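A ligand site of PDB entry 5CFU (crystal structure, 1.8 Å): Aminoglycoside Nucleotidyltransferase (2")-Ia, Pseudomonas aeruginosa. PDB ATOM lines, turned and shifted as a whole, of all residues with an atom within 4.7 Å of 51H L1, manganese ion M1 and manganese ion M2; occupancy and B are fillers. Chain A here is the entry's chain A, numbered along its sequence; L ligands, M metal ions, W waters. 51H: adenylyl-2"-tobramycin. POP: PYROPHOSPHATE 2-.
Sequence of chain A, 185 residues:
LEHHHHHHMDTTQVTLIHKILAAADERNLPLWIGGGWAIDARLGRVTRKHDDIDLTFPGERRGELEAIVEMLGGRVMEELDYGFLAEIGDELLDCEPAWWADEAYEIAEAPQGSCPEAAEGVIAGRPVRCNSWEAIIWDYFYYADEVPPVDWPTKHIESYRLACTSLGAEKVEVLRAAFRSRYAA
The side-chain amino group (NZ) of Lys 155 is in salt-bridge range of an oxygen (O6) of POP L2, 2.9 Å away. O of Ala 108 is in hydrogen-bond range of N of 51H L1, at 3.0 Å. N of Gly 36 lies close to O1 of POP L2 (3.2 Å). O4 of POP L3 lies within salt-bridge range of NZ of Lys 155 (3.9 Å). The side-chain carboxylate (OD2) of Asp 139 lies within salt-bridge range of a nitrogen (N1) of 51H L1 (2.8 Å). An oxygen (O12) of 51H L1 sits close to the side-chain hydroxyl (OH) of Tyr 140 (3.4 Å). NE2 of His 156 lies close to O of POP L2, 3.3 Å away. The backbone NH (N) of Tyr 140 is in hydrogen-bond range of an oxygen (O11) of 51H L1, at 3.1 Å. The side-chain hydroxyl of Tyr 82 lies within hydrogen-bond range of an oxygen (O2) of 51H L1 (3.4 Å). An oxygen (O11) of 51H L1 sits close to the backbone carbonyl oxygen (O) of Asp 139 (3.4 Å). The side-chain carboxylate of Glu 96 lies within salt-bridge range of a nitrogen (N1) of 51H L1. The backbone NH of Asp 51 sits at hydrogen-bond distance from an oxygen (O6) of POP L2, 2.9 Å away. The side-chain carboxylate (OD2) of Asp 51 lies close to an oxygen (O5) of POP L3 (3.1 Å). OD2 of Asp 94 is in salt-bridge range of N2 of 51H L1 (3.0 Å). N9 of 51H L1 is in salt-bridge range of OE1 of Glu 146, at 2.6 Å.
The side-chain carboxylate (OD1) of Asp 94 is in hydrogen-bond range of the side-chain hydroxyl (OH) of Tyr 82, at 2.9 Å. The side-chain hydroxyl (OH) of Tyr 140 is in hydrogen-bond range of a ring nitrogen (ND1) of His 156 (3.2 Å).
Ile 107 touches 51H L1. Tyr 142 touches 51H L1 (CE2 to O, 3.5 Å). Tyr 143 touches 51H L1. NE2 of His 156 touches C19 of 51H L1 (3.6 Å). Hydrophobic or aromatic side chains that line 51H L1: Tyr 82, Ile 107, Tyr 140, Tyr 142, Tyr 143 and His 156. Within 4 Å of 51H L1: Asp 52, Asp 54, Tyr 82, Asp 94, Glu 96, Ile 107, Ala 108, Asp 139, Tyr 140, Tyr 142, Tyr 143, Glu 146 and His 156. The nearest printed residue that does not touch 51H L1 is Ile 136 (4.2 Å).
Along chain A the residues within 4 Å of manganese ion M1 span positions 52 to 54. The nearest printed residue that does not touch manganese ion M1 is Gly 36 (4.4 Å).
His 156 touches manganese ion M2. Of the 18 residues printed, 1 comes within 4 Å of manganese ion M2.
Manganese ion M1 is bound by an oxygen (O7) of 51H L1 (2.0 Å), the side-chain carboxylate (OD1) of Asp 52 (2.0 Å), an oxygen (O3) of POP L2 (2.1 Å), an oxygen (O5) of POP L2 (2.2 Å), water W6 (2.2 Å) and the side-chain carboxylate (OD2) of Asp 54 (2.2 Å).
Manganese ion M2 is bound by an oxygen (O4) of POP L2 (1.8 Å), an oxygen (O8) of 51H L1 (1.9 Å), an oxygen (O6) of POP L3 (2.2 Å), water W3 (2.2 Å), an oxygen (O3) of POP L3 (2.2 Å) and water W7 (2.3 Å). Manganese ion M2 has six donor atoms within binding distance.
Water W6 lies within hydrogen-bond range of the backbone carbonyl oxygen of Asp 52 (2.7 Å) and an oxygen (O2) of POP L2 (2.7 Å). Water W4 lies within hydrogen-bond range of an oxygen (O12) of 51H L1 (2.5 Å), an oxygen (O1) of POP L2 (2.5 Å), the side-chain hydroxyl of Tyr 140 (2.7 Å) and the backbone NH of Gly 36 (3.3 Å). Water W2 bridges the backbone carbonyl oxygen of Ile 136 (2.7 Å) and an oxygen (O12) of 51H L1 (2.8 Å). Water W10 lies within hydrogen-bond range of the side-chain carboxylate of Asp 139 (2.6 Å) and a nitrogen (N) of 51H L1 (2.8 Å). Water W9 lies within hydrogen-bond range of O of Asp 139 (2.8 Å) and N9 of 51H L1 (2.9 Å). Water W5 bridges O of Asp 94 (2.8 Å) and N2 of 51H L1 (3.1 Å).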
ATOM      1  N   GLY A  35       0.899 -17.670  23.582  1.00  0.00           N
ATOM      2  CA  GLY A  35       1.369 -16.358  23.977  1.00  0.00           C
ATOM      3  C   GLY A  35       1.169 -15.319  22.897  1.00  0.00           C
ATOM      4  O   GLY A  35       0.129 -15.308  22.214  1.00  0.00           O
ATOM      5  N   GLY A  36       2.156 -14.433  22.745  1.00  0.00           N
ATOM      6  CA  GLY A  36       2.036 -13.301  21.837  1.00  0.00           C
ATOM      7  C   GLY A  36       1.793 -13.694  20.401  1.00  0.00           C
ATOM      8  O   GLY A  36       1.021 -13.039  19.704  1.00  0.00           O
ATOM      9  N   ASP A  51       9.440 -11.636  21.966  1.00  0.00           N
ATOM     10  CA  ASP A  51      10.751 -12.033  22.494  1.00  0.00           C
ATOM     11  C   ASP A  51      11.038 -13.489  22.214  1.00  0.00           C
ATOM     12  O   ASP A  51      12.174 -13.839  21.897  1.00  0.00           O
ATOM     13  CB  ASP A  51      10.842 -11.764  23.994  1.00  0.00           C
ATOM     14  CG  ASP A  51      11.160 -10.323  24.318  1.00  0.00           C
ATOM     15  OD1 ASP A  51      11.249  -9.510  23.369  1.00  0.00           O
ATOM     16  OD2 ASP A  51      11.328 -10.012  25.513  1.00  0.00           O
ATOM     17  N   ASP A  52      10.025 -14.336  22.308  1.00  0.00           N
ATOM     18  CA  ASP A  52      10.216 -15.773  22.097  1.00  0.00           C
ATOM     19  C   ASP A  52       9.094 -16.347  21.228  1.00  0.00           C
ATOM     20  O   ASP A  52       8.201 -15.631  20.779  1.00  0.00           O
ATOM     21  CB  ASP A  52      10.320 -16.512  23.453  1.00  0.00           C
ATOM     22  CG  ASP A  52       9.009 -16.547  24.212  1.00  0.00           C
ATOM     23  OD1 ASP A  52       8.005 -15.988  23.720  1.00  0.00           O
ATOM     24  OD2 ASP A  52       8.978 -17.123  25.323  1.00  0.00           O
ATOM     25  N   ASP A  54       6.296 -19.218  21.745  1.00  0.00           N
ATOM     26  CA  ASP A  54       5.657 -20.078  22.718  1.00  0.00           C
ATOM     27  C   ASP A  54       4.893 -21.200  22.017  1.00  0.00           C
ATOM     28  O   ASP A  54       4.109 -20.933  21.101  1.00  0.00           O
ATOM     29  CB  ASP A  54       4.710 -19.277  23.590  1.00  0.00           C
ATOM     30  CG  ASP A  54       5.409 -18.156  24.306  1.00  0.00           C
ATOM     31  OD1 ASP A  54       6.251 -18.447  25.187  1.00  0.00           O
ATOM     32  OD2 ASP A  54       5.133 -16.991  23.948  1.00  0.00           O
ATOM     33  N   TYR A  82       7.090 -25.958  34.065  1.00  0.00           N
ATOM     34  CA  TYR A  82       5.899 -26.246  33.248  1.00  0.00           C
ATOM     35  C   TYR A  82       6.224 -26.851  31.882  1.00  0.00           C
ATOM     36  O   TYR A  82       5.317 -27.103  31.090  1.00  0.00           O
ATOM     37  CB  TYR A  82       5.082 -24.956  33.054  1.00  0.00           C
ATOM     38  CG  TYR A  82       5.902 -23.869  32.384  1.00  0.00           C
ATOM     39  CD1 TYR A  82       6.105 -23.861  31.008  1.00  0.00           C
ATOM     40  CD2 TYR A  82       6.524 -22.876  33.144  1.00  0.00           C
ATOM     41  CE1 TYR A  82       6.874 -22.885  30.412  1.00  0.00           C
ATOM     42  CE2 TYR A  82       7.304 -21.907  32.541  1.00  0.00           C
ATOM     43  CZ  TYR A  82       7.470 -21.924  31.190  1.00  0.00           C
ATOM     44  OH  TYR A  82       8.227 -20.956  30.597  1.00  0.00           O
ATOM     45  N   ASP A  94       9.702 -21.579  23.859  1.00  0.00           N
ATOM     46  CA  ASP A  94       9.215 -21.844  25.211  1.00  0.00           C
ATOM     47  C   ASP A  94       8.083 -22.872  25.103  1.00  0.00           C
ATOM     48  O   ASP A  94       7.024 -22.563  24.573  1.00  0.00           O
ATOM     49  CB  ASP A  94       8.745 -20.543  25.836  1.00  0.00           C
ATOM     50  CG  ASP A  94       8.522 -20.648  27.332  1.00  0.00           C
ATOM     51  OD1 ASP A  94       9.345 -20.139  28.095  1.00  0.00           O
ATOM     52  OD2 ASP A  94       7.523 -21.247  27.747  1.00  0.00           O
ATOM     53  N   GLU A  96       5.467 -26.005  26.336  1.00  0.00           N
ATOM     54  CA  GLU A  96       4.647 -26.564  27.406  1.00  0.00           C
ATOM     55  C   GLU A  96       3.839 -27.752  26.897  1.00  0.00           C
ATOM     56  O   GLU A  96       3.217 -27.653  25.858  1.00  0.00           O
ATOM     57  CB  GLU A  96       3.690 -25.502  27.958  1.00  0.00           C
ATOM     58  CG  GLU A  96       2.764 -26.020  29.055  1.00  0.00           C
ATOM     59  CD  GLU A  96       2.028 -24.904  29.782  1.00  0.00           C
ATOM     60  OE1 GLU A  96       1.622 -23.924  29.124  1.00  0.00           O
ATOM     61  OE2 GLU A  96       1.849 -25.025  31.021  1.00  0.00           O
ATOM     62  N   ILE A 107      -3.853 -28.256  28.232  1.00  0.00           N
ATOM     63  CA  ILE A 107      -2.820 -27.755  29.114  1.00  0.00           C
ATOM     64  C   ILE A 107      -3.252 -27.978  30.558  1.00  0.00           C
ATOM     65  O   ILE A 107      -4.400 -27.684  30.915  1.00  0.00           O
ATOM     66  CB  ILE A 107      -2.551 -26.263  28.863  1.00  0.00           C
ATOM     67  CG1 ILE A 107      -1.964 -26.083  27.453  1.00  0.00           C
ATOM     68  CG2 ILE A 107      -1.651 -25.651  29.916  1.00  0.00           C
ATOM     69  CD1 ILE A 107      -2.036 -24.683  26.958  1.00  0.00           C
ATOM     70  N   ALA A 108      -2.346 -28.489  31.374  1.00  0.00           N
ATOM     71  CA  ALA A 108      -2.638 -28.687  32.787  1.00  0.00           C
ATOM     72  C   ALA A 108      -3.148 -27.385  33.455  1.00  0.00           C
ATOM     73  O   ALA A 108      -2.594 -26.314  33.215  1.00  0.00           O
ATOM     74  CB  ALA A 108      -1.398 -29.205  33.529  1.00  0.00           C
ATOM     75  N   ILE A 136      -5.002 -18.199  26.637  1.00  0.00           N
ATOM     76  CA  ILE A 136      -4.105 -17.054  26.529  1.00  0.00           C
ATOM     77  C   ILE A 136      -4.290 -16.104  27.703  1.00  0.00           C
ATOM     78  O   ILE A 136      -3.335 -15.714  28.352  1.00  0.00           O
ATOM     79  CB  ILE A 136      -4.342 -16.313  25.173  1.00  0.00           C
ATOM     80  CG1 ILE A 136      -3.865 -17.174  23.997  1.00  0.00           C
ATOM     81  CG2 ILE A 136      -3.619 -14.967  25.161  1.00  0.00           C
ATOM     82  CD1 ILE A 136      -4.365 -16.669  22.618  1.00  0.00           C
ATOM     83  N   ASP A 139      -3.241 -17.346  31.271  1.00  0.00           N
ATOM     84  CA  ASP A 139      -1.839 -17.189  31.644  1.00  0.00           C
ATOM     85  C   ASP A 139      -1.525 -15.774  32.124  1.00  0.00           C
ATOM     86  O   ASP A 139      -0.610 -15.600  32.912  1.00  0.00           O
ATOM     87  CB  ASP A 139      -0.922 -17.584  30.479  1.00  0.00           C
ATOM     88  CG  ASP A 139      -0.521 -19.058  30.522  1.00  0.00           C
ATOM     89  OD1 ASP A 139      -0.823 -19.716  31.544  1.00  0.00           O
ATOM     90  OD2 ASP A 139       0.094 -19.545  29.546  1.00  0.00           O
ATOM     91  N   TYR A 140      -2.282 -14.774  31.677  1.00  0.00           N
ATOM     92  CA  TYR A 140      -2.157 -13.423  32.258  1.00  0.00           C
ATOM     93  C   TYR A 140      -2.644 -13.364  33.685  1.00  0.00           C
ATOM     94  O   TYR A 140      -2.125 -12.586  34.497  1.00  0.00           O
ATOM     95  CB  TYR A 140      -2.919 -12.380  31.414  1.00  0.00           C
ATOM     96  CG  TYR A 140      -2.137 -11.921  30.209  1.00  0.00           C
ATOM     97  CD1 TYR A 140      -1.054 -11.078  30.358  1.00  0.00           C
ATOM     98  CD2 TYR A 140      -2.447 -12.366  28.925  1.00  0.00           C
ATOM     99  CE1 TYR A 140      -0.329 -10.665  29.265  1.00  0.00           C
ATOM    100  CE2 TYR A 140      -1.712 -11.954  27.835  1.00  0.00           C
ATOM    101  CZ  TYR A 140      -0.664 -11.100  28.007  1.00  0.00           C
ATOM    102  OH  TYR A 140       0.081 -10.688  26.918  1.00  0.00           O
ATOM    103  N   TYR A 142      -2.381 -15.880  35.905  1.00  0.00           N
ATOM    104  CA  TYR A 142      -1.220 -16.393  36.630  1.00  0.00           C
ATOM    105  C   TYR A 142      -0.145 -15.328  36.776  1.00  0.00           C
ATOM    106  O   TYR A 142       0.453 -15.166  37.844  1.00  0.00           O
ATOM    107  CB  TYR A 142      -0.604 -17.583  35.924  1.00  0.00           C
ATOM    108  CG  TYR A 142      -1.326 -18.882  36.039  1.00  0.00           C
ATOM    109  CD1 TYR A 142      -1.548 -19.462  37.282  1.00  0.00           C
ATOM    110  CD2 TYR A 142      -1.692 -19.589  34.913  1.00  0.00           C
ATOM    111  CE1 TYR A 142      -2.179 -20.686  37.370  1.00  0.00           C
ATOM    112  CE2 TYR A 142      -2.290 -20.798  34.996  1.00  0.00           C
ATOM    113  CZ  TYR A 142      -2.536 -21.345  36.211  1.00  0.00           C
ATOM    114  OH  TYR A 142      -3.167 -22.562  36.256  1.00  0.00           O
ATOM    115  N   TYR A 143       0.134 -14.649  35.671  1.00  0.00           N
ATOM    116  CA  TYR A 143       1.179 -13.636  35.611  1.00  0.00           C
ATOM    117  C   TYR A 143       0.884 -12.556  36.658  1.00  0.00           C
ATOM    118  O   TYR A 143       1.766 -12.139  37.412  1.00  0.00           O
ATOM    119  CB  TYR A 143       1.252 -13.069  34.201  1.00  0.00           C
ATOM    120  CG  TYR A 143       2.386 -12.132  33.899  1.00  0.00           C
ATOM    121  CD1 TYR A 143       3.542 -12.116  34.672  1.00  0.00           C
ATOM    122  CD2 TYR A 143       2.298 -11.254  32.833  1.00  0.00           C
ATOM    123  CE1 TYR A 143       4.567 -11.245  34.386  1.00  0.00           C
ATOM    124  CE2 TYR A 143       3.315 -10.374  32.540  1.00  0.00           C
ATOM    125  CZ  TYR A 143       4.446 -10.382  33.325  1.00  0.00           C
ATOM    126  OH  TYR A 143       5.464  -9.521  33.022  1.00  0.00           O
ATOM    127  N   GLU A 146       1.888 -13.952  40.117  1.00  0.00           N
ATOM    128  CA  GLU A 146       3.337 -14.142  40.239  1.00  0.00           C
ATOM    129  C   GLU A 146       4.107 -12.819  40.241  1.00  0.00           C
ATOM    130  O   GLU A 146       5.137 -12.691  40.908  1.00  0.00           O
ATOM    131  CB  GLU A 146       3.824 -15.051  39.102  1.00  0.00           C
ATOM    132  CG  GLU A 146       3.177 -16.438  39.131  1.00  0.00           C
ATOM    133  CD  GLU A 146       3.483 -17.279  37.898  1.00  0.00           C
ATOM    134  OE1 GLU A 146       2.729 -18.247  37.612  1.00  0.00           O
ATOM    135  OE2 GLU A 146       4.493 -16.980  37.217  1.00  0.00           O
ATOM    136  N   LYS A 155       4.553  -3.883  27.361  1.00  0.00           N
ATOM    137  CA  LYS A 155       4.154  -4.708  26.216  1.00  0.00           C
ATOM    138  C   LYS A 155       3.128  -5.784  26.652  1.00  0.00           C
ATOM    139  O   LYS A 155       2.337  -6.257  25.843  1.00  0.00           O
ATOM    140  CB  LYS A 155       5.354  -5.386  25.575  1.00  0.00           C
ATOM    141  CG  LYS A 155       6.023  -6.423  26.473  1.00  0.00           C
ATOM    142  CD  LYS A 155       7.130  -7.203  25.765  1.00  0.00           C
ATOM    143  CE  LYS A 155       7.731  -8.258  26.690  1.00  0.00           C
ATOM    144  NZ  LYS A 155       8.803  -9.062  26.043  1.00  0.00           N
ATOM    145  N   HIS A 156       3.145  -6.156  27.923  1.00  0.00           N
ATOM    146  CA  HIS A 156       2.205  -7.182  28.400  1.00  0.00           C
ATOM    147  C   HIS A 156       0.916  -6.590  28.913  1.00  0.00           C
ATOM    148  O   HIS A 156      -0.133  -7.209  28.793  1.00  0.00           O
ATOM    149  CB  HIS A 156       2.858  -8.052  29.461  1.00  0.00           C
ATOM    150  CG  HIS A 156       3.611  -9.180  28.846  1.00  0.00           C
ATOM    151  ND1 HIS A 156       3.029 -10.032  27.927  1.00  0.00           N
ATOM    152  CD2 HIS A 156       4.903  -9.556  28.940  1.00  0.00           C
ATOM    153  CE1 HIS A 156       3.926 -10.900  27.511  1.00  0.00           C
ATOM    154  NE2 HIS A 156       5.071 -10.633  28.108  1.00  0.00           N
HETATM  155  O8  51H L   1       7.043 -14.050  28.070  1.00  0.00           O
HETATM  156  P   51H L   1       6.213 -15.185  27.631  1.00  0.00           P
HETATM  157  O7  51H L   1       6.284 -15.506  26.172  1.00  0.00           O
HETATM  158  O9  51H L   1       4.706 -14.936  27.981  1.00  0.00           O
HETATM  159  C14 51H L   1       3.673 -15.838  27.534  1.00  0.00           C
HETATM  160  C15 51H L   1       2.463 -15.523  28.379  1.00  0.00           C
HETATM  161  C18 51H L   1       2.052 -14.062  28.332  1.00  0.00           C
HETATM  162  O12 51H L   1       1.005 -13.893  27.379  1.00  0.00           O
HETATM  163  C17 51H L   1       1.576 -13.781  29.760  1.00  0.00           C
HETATM  164  O11 51H L   1       0.202 -14.120  29.928  1.00  0.00           O
HETATM  165  C16 51H L   1       2.439 -14.736  30.582  1.00  0.00           C
HETATM  166  N4  51H L   1       3.670 -14.160  31.080  1.00  0.00           N
HETATM  167  C21 51H L   1       4.304 -14.489  32.253  1.00  0.00           C
HETATM  168  N6  51H L   1       3.866 -15.320  33.203  1.00  0.00           N
HETATM  169  C22 51H L   1       4.741 -15.403  34.212  1.00  0.00           C
HETATM  170  N7  51H L   1       5.921 -14.794  34.337  1.00  0.00           N
HETATM  171  C23 51H L   1       6.343 -13.961  33.369  1.00  0.00           C
HETATM  172  N8  51H L   1       7.531 -13.374  33.500  1.00  0.00           N
HETATM  173  C20 51H L   1       5.494 -13.782  32.257  1.00  0.00           C
HETATM  174  N5  51H L   1       5.612 -13.010  31.116  1.00  0.00           N
HETATM  175  C19 51H L   1       4.502 -13.267  30.455  1.00  0.00           C
HETATM  176  O10 51H L   1       2.770 -15.822  29.748  1.00  0.00           O
HETATM  177  O6  51H L   1       6.582 -16.503  28.432  1.00  0.00           O
HETATM  178  C13 51H L   1       7.020 -16.410  29.798  1.00  0.00           C
HETATM  179  C12 51H L   1       8.450 -16.910  29.895  1.00  0.00           C
HETATM  180  N3  51H L   1       9.320 -16.153  28.964  1.00  0.00           N
HETATM  181  C11 51H L   1       8.934 -16.823  31.337  1.00  0.00           C
HETATM  182  O5  51H L   1      10.258 -17.317  31.448  1.00  0.00           O
HETATM  183  C9  51H L   1       7.973 -17.652  32.193  1.00  0.00           C
HETATM  184  C10 51H L   1       8.304 -17.625  33.663  1.00  0.00           C
HETATM  185  O4  51H L   1       7.610 -18.650  34.334  1.00  0.00           O
HETATM  186  O3  51H L   1       6.629 -17.157  32.077  1.00  0.00           O
HETATM  187  C8  51H L   1       6.114 -17.170  30.750  1.00  0.00           C
HETATM  188  O2  51H L   1       5.987 -18.475  30.285  1.00  0.00           O
HETATM  189  C7  51H L   1       4.680 -19.066  30.326  1.00  0.00           C
HETATM  190  C6  51H L   1       4.650 -20.167  29.262  1.00  0.00           C
HETATM  191  N2  51H L   1       5.041 -19.627  27.940  1.00  0.00           N
HETATM  192  C5  51H L   1       3.266 -20.782  29.230  1.00  0.00           C
HETATM  193  C4  51H L   1       2.851 -21.353  30.608  1.00  0.00           C
HETATM  194  N1  51H L   1       1.457 -21.800  30.564  1.00  0.00           N
HETATM  195  C24 51H L   1       4.381 -19.644  31.691  1.00  0.00           C
HETATM  196  O13 51H L   1       4.396 -18.635  32.707  1.00  0.00           O
HETATM  197  C3  51H L   1       3.000 -20.277  31.687  1.00  0.00           C
HETATM  198  O1  51H L   1       2.779 -20.912  32.958  1.00  0.00           O
HETATM  199  C2  51H L   1       1.547 -20.705  33.590  1.00  0.00           C
HETATM  200  O   51H L   1       0.726 -21.853  33.488  1.00  0.00           O
HETATM  201  C25 51H L   1       1.804 -20.332  35.056  1.00  0.00           C
HETATM  202  N9  51H L   1       2.692 -19.176  35.189  1.00  0.00           N
HETATM  203  C26 51H L   1       2.394 -21.571  35.751  1.00  0.00           C
HETATM  204  C27 51H L   1       1.518 -22.789  35.602  1.00  0.00           C
HETATM  205  O14 51H L   1       2.153 -23.955  36.150  1.00  0.00           O
HETATM  206  C1  51H L   1       1.205 -23.054  34.134  1.00  0.00           C
HETATM  207  C   51H L   1       0.135 -24.109  33.969  1.00  0.00           C
HETATM  208  N   51H L   1      -0.405 -24.333  32.618  1.00  0.00           N
HETATM  209  P1  POP L   2       4.501 -12.490  24.040  1.00  0.00           P
HETATM  210  O1  POP L   2       3.155 -11.820  24.259  1.00  0.00           O
HETATM  211  O2  POP L   2       5.066 -12.284  22.644  1.00  0.00           O
HETATM  212  O3  POP L   2       4.570 -13.934  24.541  1.00  0.00           O
HETATM  213  O   POP L   2       5.487 -11.639  24.981  1.00  0.00           O
HETATM  214  P2  POP L   2       7.088 -11.865  25.007  1.00  0.00           P
HETATM  215  O4  POP L   2       7.446 -11.612  26.454  1.00  0.00           O
HETATM  216  O5  POP L   2       7.355 -13.248  24.456  1.00  0.00           O
HETATM  217  O6  POP L   2       7.619 -10.807  24.056  1.00  0.00           O
HETATM  218  P1  POP L   3      10.391 -13.070  30.444  1.00  0.00           P
HETATM  219  O1  POP L   3       9.692 -12.615  31.704  1.00  0.00           O
HETATM  220  O2  POP L   3      11.516 -14.052  30.705  1.00  0.00           O
HETATM  221  O3  POP L   3       9.425 -13.553  29.397  1.00  0.00           O
HETATM  222  O   POP L   3      11.107 -11.708  29.942  1.00  0.00           O
HETATM  223  P2  POP L   3      11.221 -11.099  28.445  1.00  0.00           P
HETATM  224  O4  POP L   3      11.642  -9.665  28.666  1.00  0.00           O
HETATM  225  O5  POP L   3      12.261 -11.945  27.748  1.00  0.00           O
HETATM  226  O6  POP L   3       9.840 -11.170  27.849  1.00  0.00           O
HETATM  227 MN    MN M   1       6.251 -15.087  24.224  1.00  0.00          MN
HETATM  228 MN    MN M   2       8.212 -12.604  27.814  1.00  0.00          MN
HETATM  229  O   HOH W   1      10.718 -19.877  31.161  1.00  0.00           O
HETATM  230  O   HOH W   2      -0.902 -15.856  27.095  1.00  0.00           O
HETATM  231  O   HOH W   3       9.209 -13.948  26.397  1.00  0.00           O
HETATM  232  O   HOH W   4       0.959 -12.619  25.249  1.00  0.00           O
HETATM  233  O   HOH W   5       4.896 -22.247  26.358  1.00  0.00           O
HETATM  234  O   HOH W   6       6.005 -14.771  22.050  1.00  0.00           O
HETATM  235  O   HOH W   7       7.411 -11.448  29.618  1.00  0.00           O
HETATM  236  O   HOH W   8       4.814 -24.060  36.753  1.00  0.00           O
HETATM  237  O   HOH W   9       1.616 -17.327  33.217  1.00  0.00           O
HETATM  238  O   HOH W  10      -1.852 -22.133  31.551  1.00  0.00           O
HETATM  239  O   HOH W  11       2.888 -18.868  26.455  1.00  0.00           O
